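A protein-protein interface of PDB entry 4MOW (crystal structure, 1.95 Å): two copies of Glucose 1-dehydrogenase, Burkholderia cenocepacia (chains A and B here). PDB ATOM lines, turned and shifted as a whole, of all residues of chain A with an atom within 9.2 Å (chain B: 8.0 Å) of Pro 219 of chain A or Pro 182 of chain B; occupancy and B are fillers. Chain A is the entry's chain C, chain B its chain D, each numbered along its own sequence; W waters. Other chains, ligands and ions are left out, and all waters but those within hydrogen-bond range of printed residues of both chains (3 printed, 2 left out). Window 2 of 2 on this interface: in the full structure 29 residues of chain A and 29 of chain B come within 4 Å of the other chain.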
ATOM      1  N   GLN A 213      15.526 -14.672  11.211  1.00  0.00           N
ATOM      2  CA  GLN A 213      15.574 -15.794  12.127  1.00  0.00           C
ATOM      3  C   GLN A 213      14.560 -16.875  11.676  1.00  0.00           C
ATOM      4  O   GLN A 213      14.867 -18.074  11.607  1.00  0.00           O
ATOM      5  CB  GLN A 213      15.276 -15.345  13.556  1.00  0.00           C
ATOM      6  N   VAL A 214      13.360 -16.440  11.335  1.00  0.00           N
ATOM      7  CA  VAL A 214      12.331 -17.404  11.034  1.00  0.00           C
ATOM      8  C   VAL A 214      12.674 -18.090   9.727  1.00  0.00           C
ATOM      9  O   VAL A 214      12.485 -19.278   9.580  1.00  0.00           O
ATOM     10  CB  VAL A 214      10.956 -16.752  10.974  1.00  0.00           C
ATOM     11  CG1 VAL A 214       9.915 -17.763  10.499  1.00  0.00           C
ATOM     12  CG2 VAL A 214      10.579 -16.195  12.341  1.00  0.00           C
ATOM     13  N   LEU A 215      13.210 -17.327   8.796  1.00  0.00           N
ATOM     14  CA  LEU A 215      13.597 -17.875   7.531  1.00  0.00           C
ATOM     15  C   LEU A 215      14.617 -18.972   7.731  1.00  0.00           C
ATOM     16  O   LEU A 215      14.511 -20.038   7.106  1.00  0.00           O
ATOM     17  CB  LEU A 215      14.149 -16.787   6.641  1.00  0.00           C
ATOM     18  CG  LEU A 215      14.665 -17.139   5.257  1.00  0.00           C
ATOM     19  CD1 LEU A 215      13.691 -17.981   4.457  1.00  0.00           C
ATOM     20  CD2 LEU A 215      14.955 -15.826   4.523  1.00  0.00           C
ATOM     21  N   GLY A 216      15.589 -18.725   8.611  1.00  0.00           N
ATOM     22  CA  GLY A 216      16.635 -19.712   8.888  1.00  0.00           C
ATOM     23  C   GLY A 216      16.139 -21.001   9.534  1.00  0.00           C
ATOM     24  O   GLY A 216      16.810 -22.034   9.474  1.00  0.00           O
ATOM     25  N   GLN A 217      14.968 -20.956  10.165  1.00  0.00           N
ATOM     26  CA  GLN A 217      14.389 -22.148  10.767  1.00  0.00           C
ATOM     27  C   GLN A 217      13.319 -22.796   9.882  1.00  0.00           C
ATOM     28  O   GLN A 217      12.658 -23.737  10.314  1.00  0.00           O
ATOM     29  CB  GLN A 217      13.774 -21.791  12.117  1.00  0.00           C
ATOM     30  CG  GLN A 217      14.752 -21.205  13.116  1.00  0.00           C
ATOM     31  CD  GLN A 217      14.050 -20.591  14.326  1.00  0.00           C
ATOM     32  OE1 GLN A 217      13.337 -19.576  14.213  1.00  0.00           O
ATOM     33  NE2 GLN A 217      14.244 -21.205  15.494  1.00  0.00           N
ATOM     34  N   THR A 218      13.125 -22.287   8.662  1.00  0.00           N
ATOM     35  CA  THR A 218      12.051 -22.756   7.796  1.00  0.00           C
ATOM     36  C   THR A 218      12.603 -23.689   6.728  1.00  0.00           C
ATOM     37  O   THR A 218      13.252 -23.222   5.780  1.00  0.00           O
ATOM     38  CB  THR A 218      11.298 -21.579   7.136  1.00  0.00           C
ATOM     39  OG1 THR A 218      10.731 -20.766   8.136  1.00  0.00           O
ATOM     40  CG2 THR A 218      10.191 -22.036   6.250  1.00  0.00           C
ATOM     41  N   PRO A 219      12.341 -25.002   6.869  1.00  0.00           N
ATOM     42  CA  PRO A 219      12.902 -25.975   5.938  1.00  0.00           C
ATOM     43  C   PRO A 219      12.667 -25.676   4.454  1.00  0.00           C
ATOM     44  O   PRO A 219      13.538 -25.990   3.655  1.00  0.00           O
ATOM     45  CB  PRO A 219      12.200 -27.282   6.304  1.00  0.00           C
ATOM     46  CG  PRO A 219      11.816 -27.133   7.739  1.00  0.00           C
ATOM     47  CD  PRO A 219      11.607 -25.660   7.984  1.00  0.00           C
ATOM     48  N   LEU A 220      11.523 -25.103   4.070  1.00  0.00           N
ATOM     49  CA  LEU A 220      11.221 -24.897   2.617  1.00  0.00           C
ATOM     50  C   LEU A 220      11.770 -23.586   2.070  1.00  0.00           C
ATOM     51  O   LEU A 220      11.445 -23.210   0.935  1.00  0.00           O
ATOM     52  CB  LEU A 220       9.721 -25.007   2.325  1.00  0.00           C
ATOM     53  CG  LEU A 220       9.207 -26.448   2.469  1.00  0.00           C
ATOM     54  CD1 LEU A 220       7.707 -26.477   2.221  1.00  0.00           C
ATOM     55  CD2 LEU A 220       9.948 -27.373   1.513  1.00  0.00           C
ATOM     56  N   GLY A 221      12.544 -22.855   2.879  1.00  0.00           N
ATOM     57  CA  GLY A 221      13.454 -21.849   2.331  1.00  0.00           C
ATOM     58  C   GLY A 221      12.843 -20.535   1.882  1.00  0.00           C
ATOM     59  O   GLY A 221      13.398 -19.873   1.009  1.00  0.00           O
ATOM     60  N   ARG A 222      11.730 -20.141   2.479  1.00  0.00           N
ATOM     61  CA  ARG A 222      11.133 -18.851   2.197  1.00  0.00           C
ATOM     62  C   ARG A 222      10.186 -18.512   3.318  1.00  0.00           C
ATOM     63  O   ARG A 222       9.937 -19.341   4.183  1.00  0.00           O
ATOM     64  CB  ARG A 222      10.439 -18.790   0.806  1.00  0.00           C
ATOM     65  CG  ARG A 222       9.304 -19.794   0.533  1.00  0.00           C
ATOM     66  CD  ARG A 222       8.400 -19.329  -0.600  1.00  0.00           C
ATOM     67  NE  ARG A 222       7.320 -20.272  -0.880  1.00  0.00           N
ATOM     68  CZ  ARG A 222       6.068 -20.197  -0.411  1.00  0.00           C
ATOM     69  NH1 ARG A 222       5.698 -19.207   0.391  1.00  0.00           N
ATOM     70  NH2 ARG A 222       5.158 -21.104  -0.784  1.00  0.00           N
ATOM     71  N   LEU A 223       9.661 -17.297   3.314  1.00  0.00           N
ATOM     72  CA  LEU A 223       8.618 -16.967   4.259  1.00  0.00           C
ATOM     73  C   LEU A 223       7.260 -17.252   3.616  1.00  0.00           C
ATOM     74  O   LEU A 223       7.106 -17.316   2.375  1.00  0.00           O
ATOM     75  CB  LEU A 223       8.708 -15.511   4.701  1.00  0.00           C
ATOM     76  CG  LEU A 223       9.931 -15.153   5.542  1.00  0.00           C
ATOM     77  CD1 LEU A 223       9.975 -13.661   5.817  1.00  0.00           C
ATOM     78  CD2 LEU A 223       9.959 -15.936   6.847  1.00  0.00           C
ATOM     79  N   SER A 252       3.539 -23.897   7.730  1.00  0.00           N
ATOM     80  CA  SER A 252       4.665 -23.042   8.149  1.00  0.00           C
ATOM     81  C   SER A 252       5.938 -23.265   7.322  1.00  0.00           C
ATOM     82  O   SER A 252       6.998 -22.826   7.721  1.00  0.00           O
ATOM     83  CB  SER A 252       5.010 -23.338   9.594  1.00  0.00           C
ATOM     84  OG  SER A 252       5.556 -24.640   9.807  1.00  0.00           O
ATOM     85  N   GLY A 253       5.829 -24.059   6.260  1.00  0.00           N
ATOM     86  CA  GLY A 253       6.974 -24.489   5.494  1.00  0.00           C
ATOM     87  C   GLY A 253       7.886 -25.463   6.185  1.00  0.00           C
ATOM     88  O   GLY A 253       9.098 -25.529   5.869  1.00  0.00           O
ATOM     89  N   GLY A 254       7.327 -26.250   7.118  1.00  0.00           N
ATOM     90  CA  GLY A 254       8.125 -27.212   7.813  1.00  0.00           C
ATOM     91  C   GLY A 254       8.578 -26.846   9.201  1.00  0.00           C
ATOM     92  O   GLY A 254       9.171 -27.667   9.806  1.00  0.00           O
ATOM     93  N   LEU A 255       8.297 -25.632   9.700  1.00  0.00           N
ATOM     94  CA  LEU A 255       8.716 -25.260  11.045  1.00  0.00           C
ATOM     95  C   LEU A 255       7.716 -25.782  12.090  1.00  0.00           C
ATOM     96  O   LEU A 255       6.556 -25.504  12.012  1.00  0.00           O
ATOM     97  CB  LEU A 255       8.880 -23.736  11.149  1.00  0.00           C
ATOM     98  CG  LEU A 255       9.185 -23.186  12.546  1.00  0.00           C
ATOM     99  CD1 LEU A 255      10.488 -23.735  13.112  1.00  0.00           C
ATOM    100  CD2 LEU A 255       9.232 -21.681  12.449  1.00  0.00           C
ATOM    101  N   ASN A 256       8.180 -26.582  13.029  1.00  0.00           N
ATOM    102  CA  ASN A 256       7.376 -27.044  14.163  1.00  0.00           C
ATOM    103  C   ASN A 256       8.257 -27.337  15.359  1.00  0.00           C
ATOM    104  O   ASN A 256       9.486 -27.173  15.293  1.00  0.00           O
ATOM    105  CB  ASN A 256       6.572 -28.306  13.788  1.00  0.00           C
ATOM    106  CG  ASN A 256       7.458 -29.459  13.349  1.00  0.00           C
ATOM    107  OD1 ASN A 256       8.472 -29.747  13.973  1.00  0.00           O
ATOM    108  ND2 ASN A 256       7.114 -30.090  12.243  1.00  0.00           N
ATOM    109  OXT ASN A 256       7.778 -27.791  16.418  1.00  0.00           O
ATOM    110  N   GLU B 140      12.540 -29.348  -7.107  1.00  0.00           N
ATOM    111  CA  GLU B 140      11.717 -28.324  -6.459  1.00  0.00           C
ATOM    112  C   GLU B 140      10.218 -28.544  -6.716  1.00  0.00           C
ATOM    113  O   GLU B 140       9.785 -28.711  -7.859  1.00  0.00           O
ATOM    114  CB  GLU B 140      12.141 -26.913  -6.884  1.00  0.00           C
ATOM    115  N   GLY B 174       9.014 -36.969   9.334  1.00  0.00           N
ATOM    116  CA  GLY B 174       9.555 -35.784   9.942  1.00  0.00           C
ATOM    117  C   GLY B 174      11.028 -35.580   9.531  1.00  0.00           C
ATOM    118  O   GLY B 174      11.469 -34.446   9.236  1.00  0.00           O
ATOM    119  N   LEU B 176      12.749 -36.760   6.879  1.00  0.00           N
ATOM    120  CA  LEU B 176      12.926 -36.423   5.467  1.00  0.00           C
ATOM    121  C   LEU B 176      12.359 -35.038   5.072  1.00  0.00           C
ATOM    122  O   LEU B 176      12.889 -34.362   4.143  1.00  0.00           O
ATOM    123  CB  LEU B 176      12.372 -37.531   4.562  1.00  0.00           C
ATOM    124  CG  LEU B 176      13.022 -38.905   4.794  1.00  0.00           C
ATOM    125  CD1 LEU B 176      12.381 -39.928   3.901  1.00  0.00           C
ATOM    126  CD2 LEU B 176      14.521 -38.816   4.544  1.00  0.00           C
ATOM    127  N   ALA B 177      11.298 -34.598   5.738  1.00  0.00           N
ATOM    128  CA  ALA B 177      10.833 -33.219   5.543  1.00  0.00           C
ATOM    129  C   ALA B 177      11.985 -32.205   5.803  1.00  0.00           C
ATOM    130  O   ALA B 177      12.201 -31.241   5.049  1.00  0.00           O
ATOM    131  CB  ALA B 177       9.660 -32.919   6.482  1.00  0.00           C
ATOM    132  N   LEU B 178      12.720 -32.414   6.887  1.00  0.00           N
ATOM    133  CA  LEU B 178      13.834 -31.534   7.217  1.00  0.00           C
ATOM    134  C   LEU B 178      15.033 -31.791   6.309  1.00  0.00           C
ATOM    135  O   LEU B 178      15.705 -30.848   5.920  1.00  0.00           O
ATOM    136  CB  LEU B 178      14.272 -31.687   8.658  1.00  0.00           C
ATOM    137  CG  LEU B 178      13.262 -31.356   9.760  1.00  0.00           C
ATOM    138  CD1 LEU B 178      13.916 -31.120  11.108  1.00  0.00           C
ATOM    139  CD2 LEU B 178      12.505 -30.109   9.363  1.00  0.00           C
ATOM    140  N   GLU B 179      15.301 -33.054   6.009  1.00  0.00           N
ATOM    141  CA  GLU B 179      16.437 -33.440   5.190  1.00  0.00           C
ATOM    142  C   GLU B 179      16.312 -32.967   3.749  1.00  0.00           C
ATOM    143  O   GLU B 179      17.308 -32.597   3.122  1.00  0.00           O
ATOM    144  CB  GLU B 179      16.610 -34.953   5.201  1.00  0.00           C
ATOM    145  CG  GLU B 179      17.971 -35.440   4.675  1.00  0.00           C
ATOM    146  CD  GLU B 179      18.179 -36.935   4.890  1.00  0.00           C
ATOM    147  OE1 GLU B 179      18.532 -37.600   3.903  1.00  0.00           O
ATOM    148  OE2 GLU B 179      17.990 -37.456   6.040  1.00  0.00           O
ATOM    149  N   LEU B 180      15.103 -33.050   3.192  1.00  0.00           N
ATOM    150  CA  LEU B 180      14.868 -32.676   1.788  1.00  0.00           C
ATOM    151  C   LEU B 180      14.306 -31.237   1.610  1.00  0.00           C
ATOM    152  O   LEU B 180      14.154 -30.723   0.462  1.00  0.00           O
ATOM    153  CB  LEU B 180      13.973 -33.739   1.144  1.00  0.00           C
ATOM    154  CG  LEU B 180      14.404 -35.202   1.339  1.00  0.00           C
ATOM    155  CD1 LEU B 180      13.389 -36.073   0.672  1.00  0.00           C
ATOM    156  CD2 LEU B 180      15.789 -35.474   0.736  1.00  0.00           C
ATOM    157  N   GLY B 181      13.987 -30.587   2.735  1.00  0.00           N
ATOM    158  CA  GLY B 181      13.613 -29.189   2.743  1.00  0.00           C
ATOM    159  C   GLY B 181      14.472 -28.294   1.837  1.00  0.00           C
ATOM    160  O   GLY B 181      13.922 -27.582   0.984  1.00  0.00           O
ATOM    161  N   PRO B 182      15.807 -28.321   2.020  1.00  0.00           N
ATOM    162  CA  PRO B 182      16.709 -27.520   1.137  1.00  0.00           C
ATOM    163  C   PRO B 182      16.504 -27.753  -0.359  1.00  0.00           C
ATOM    164  O   PRO B 182      16.621 -26.807  -1.122  1.00  0.00           O
ATOM    165  CB  PRO B 182      18.102 -27.939   1.577  1.00  0.00           C
ATOM    166  CG  PRO B 182      17.945 -28.312   3.024  1.00  0.00           C
ATOM    167  CD  PRO B 182      16.542 -28.884   3.175  1.00  0.00           C
ATOM    168  N   ARG B 183      16.143 -28.966  -0.763  1.00  0.00           N
ATOM    169  CA  ARG B 183      15.778 -29.276  -2.160  1.00  0.00           C
ATOM    170  C   ARG B 183      14.330 -28.927  -2.508  1.00  0.00           C
ATOM    171  O   ARG B 183      13.901 -29.145  -3.633  1.00  0.00           O
ATOM    172  CB  ARG B 183      16.015 -30.748  -2.463  1.00  0.00           C
ATOM    173  CG  ARG B 183      17.476 -31.059  -2.729  1.00  0.00           C
ATOM    174  CD  ARG B 183      17.774 -32.552  -2.680  1.00  0.00           C
ATOM    175  NE  ARG B 183      18.219 -32.911  -1.324  1.00  0.00           N
ATOM    176  CZ  ARG B 183      18.657 -34.120  -0.940  1.00  0.00           C
ATOM    177  NH1 ARG B 183      18.689 -35.154  -1.791  1.00  0.00           N
ATOM    178  NH2 ARG B 183      19.056 -34.294   0.321  1.00  0.00           N
ATOM    179  N   LYS B 184      13.571 -28.418  -1.534  1.00  0.00           N
ATOM    180  CA  LYS B 184      12.162 -28.074  -1.725  1.00  0.00           C
ATOM    181  C   LYS B 184      11.312 -29.262  -2.104  1.00  0.00           C
ATOM    182  O   LYS B 184      10.335 -29.114  -2.842  1.00  0.00           O
ATOM    183  CB  LYS B 184      12.003 -26.983  -2.785  1.00  0.00           C
ATOM    184  CG  LYS B 184      12.962 -25.826  -2.617  1.00  0.00           C
ATOM    185  CD  LYS B 184      12.379 -24.695  -1.783  1.00  0.00           C
ATOM    186  CE  LYS B 184      13.124 -23.399  -2.079  1.00  0.00           C
ATOM    187  NZ  LYS B 184      14.575 -23.598  -1.861  1.00  0.00           N
ATOM    188  N   ILE B 185      11.685 -30.457  -1.642  1.00  0.00           N
ATOM    189  CA  ILE B 185      10.845 -31.614  -1.810  1.00  0.00           C
ATOM    190  C   ILE B 185      10.033 -31.712  -0.488  1.00  0.00           C
ATOM    191  O   ILE B 185      10.623 -31.755   0.602  1.00  0.00           O
ATOM    192  CB  ILE B 185      11.637 -32.905  -1.990  1.00  0.00           C
ATOM    193  CG1 ILE B 185      12.556 -32.843  -3.237  1.00  0.00           C
ATOM    194  CG2 ILE B 185      10.701 -34.076  -2.138  1.00  0.00           C
ATOM    195  CD1 ILE B 185      13.809 -33.666  -3.031  1.00  0.00           C
ATOM    196  N   TRP B 243       2.953 -25.199   1.239  1.00  0.00           N
ATOM    197  CA  TRP B 243       3.546 -24.688   2.498  1.00  0.00           C
ATOM    198  C   TRP B 243       3.427 -25.668   3.695  1.00  0.00           C
ATOM    199  O   TRP B 243       3.560 -25.265   4.863  1.00  0.00           O
ATOM    200  CB  TRP B 243       2.946 -23.319   2.826  1.00  0.00           C
ATOM    201  CG  TRP B 243       3.891 -22.433   3.601  1.00  0.00           C
ATOM    202  CD1 TRP B 243       3.638 -21.719   4.743  1.00  0.00           C
ATOM    203  CD2 TRP B 243       5.229 -22.215   3.291  1.00  0.00           C
ATOM    204  NE1 TRP B 243       4.748 -21.045   5.132  1.00  0.00           N
ATOM    205  CE2 TRP B 243       5.754 -21.361   4.268  1.00  0.00           C
ATOM    206  CE3 TRP B 243       6.062 -22.678   2.275  1.00  0.00           C
ATOM    207  CZ2 TRP B 243       7.051 -20.946   4.249  1.00  0.00           C
ATOM    208  CZ3 TRP B 243       7.355 -22.281   2.277  1.00  0.00           C
ATOM    209  CH2 TRP B 243       7.840 -21.431   3.262  1.00  0.00           C
ATOM    210  N   THR B 245       5.064 -29.320   5.133  1.00  0.00           N
ATOM    211  CA  THR B 245       5.955 -30.432   5.120  1.00  0.00           C
ATOM    212  C   THR B 245       6.231 -30.921   6.533  1.00  0.00           C
ATOM    213  O   THR B 245       6.250 -30.117   7.465  1.00  0.00           O
ATOM    214  CB  THR B 245       7.267 -30.118   4.320  1.00  0.00           C
ATOM    215  OG1 THR B 245       7.929 -31.334   3.966  1.00  0.00           O
ATOM    216  CG2 THR B 245       8.178 -29.185   5.037  1.00  0.00           C
ATOM    217  N   GLY B 246       6.349 -32.257   6.668  1.00  0.00           N
ATOM    218  CA  GLY B 246       6.597 -32.880   7.950  1.00  0.00           C
ATOM    219  C   GLY B 246       5.307 -33.095   8.757  1.00  0.00           C
ATOM    220  O   GLY B 246       5.358 -33.410   9.939  1.00  0.00           O
HETATM  221  O   HOH W   1       7.464 -33.141  11.442  1.00  0.00           O
HETATM  222  O   HOH W   2       8.905 -30.343   9.000  1.00  0.00           O
HETATM  223  O   HOH W   3       5.272 -29.121   9.806  1.00  0.00           O
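Printed residues of chain A within 4 Å of Pro 182 of chain B: Pro 219 (3.6 Å).
Of the printed residues of chain A, Thr 245 of chain B touches Leu 220 (3.9 Å), Gly 253 (3.9 Å) and Gly 254 (3.4 Å).
Of the printed residues of chain A, Leu 178 of chain B touches Pro 219.
Of the printed residues of chain A, Trp 243 of chain B touches Thr 218, Leu 220, Arg 222, Leu 223, Ser 252 and Gly 253.
Leu 215 of chain A touches none of the printed residues of chain B.
The nearest residue of chain B that does not touch Pro 219 of chain A is Ala 177 of chain B (4.2 Å).
The nearest printed residue of chain B that does not touch Ser 252 of chain A is Thr 245 of chain B (6.0 Å).
Of the 16 printed residues of chain A, 8 touch a printed residue of chain B.
Hydrophobic or aromatic side chains of chain A within 4 Å of the printed part of chain B: Pro 219 and Leu 220.
Hydrophobic or aromatic side chains of chain B within 4 Å of the printed part of chain A: Leu 178 and Trp 243.
Among the printed residues, no Asp or Glu carboxylate lies within 4 Å of a Lys or Arg side-chain nitrogen of the other chain.
No position is printed for both chains.
The backbone NH (N) of Ser 252 of chain A is in hydrogen-bond range of the backbone carbonyl oxygen (O) of Trp 243 of chain B, at 3.2 Å.
The backbone NH (N) of Gly 253 of chain A lies within hydrogen-bond range of the backbone carbonyl oxygen (O) of Trp 243 of chain B (2.9 Å).
The backbone carbonyl oxygen (O) of Pro 219 of chain A lies close to the backbone carbonyl oxygen (O) of Gly 181 of chain B, at 3.1 Å.
Trp 243 of chain B touches Thr 218 of chain A.
CG of Pro 219 of chain A touches CD2 of Leu 178 of chain B, 3.5 Å away.
Pro 182 of chain B touches Pro 219 of chain A.
Lys 184 of chain B touches Leu 220 of chain A (CD to O, 3.2 Å).
Trp 243 of chain B touches Leu 220 of chain A (CZ3 to CB, 3.6 Å).
CG2 of Thr 245 of chain B touches CG of Leu 220 of chain A (3.9 Å).
O of Arg 222 of chain A touches CH2 of Trp 243 of chain B, 3.1 Å away.
Trp 243 of chain B touches Leu 223 of chain A (CZ2 to C, 3.8 Å).
Thr 245 of chain B touches Gly 253 of chain A (CG2 to O, 3.9 Å).
Thr 245 of chain B touches Gly 254 of chain A (CG2 to CA, 3.4 Å).
The backbone carbonyl oxygen (O) of Val 214 of chain A lies within hydrogen-bond range of the side-chain hydroxyl (OG1) of Thr 218 of chain A, 2.7 Å away.
The backbone NH (N) of Leu 220 of chain A is in hydrogen-bond range of the backbone carbonyl oxygen (O) of Gly 253 of chain A, at 3.0 Å.
The side-chain hydroxyl (OG) of Ser 252 of chain A is in hydrogen-bond range of the backbone carbonyl oxygen (O) of Leu 255 of chain A.
Water W1 lies within hydrogen-bond range of O of Gly 246 of chain B (2.6 Å) and ND2 of Asn 256 of chain A (3.2 Å).
Water W3 lies within hydrogen-bond range of O of Thr 245 of chain B (2.7 Å) and ND2 of Asn 256 of chain A (3.2 Å).
Water W2 lies within hydrogen-bond range of the backbone carbonyl oxygen (O) of Gly 254 of chain A (2.8 Å) and the backbone carbonyl oxygen (O) of Thr 245 of chain B (3.1 Å).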
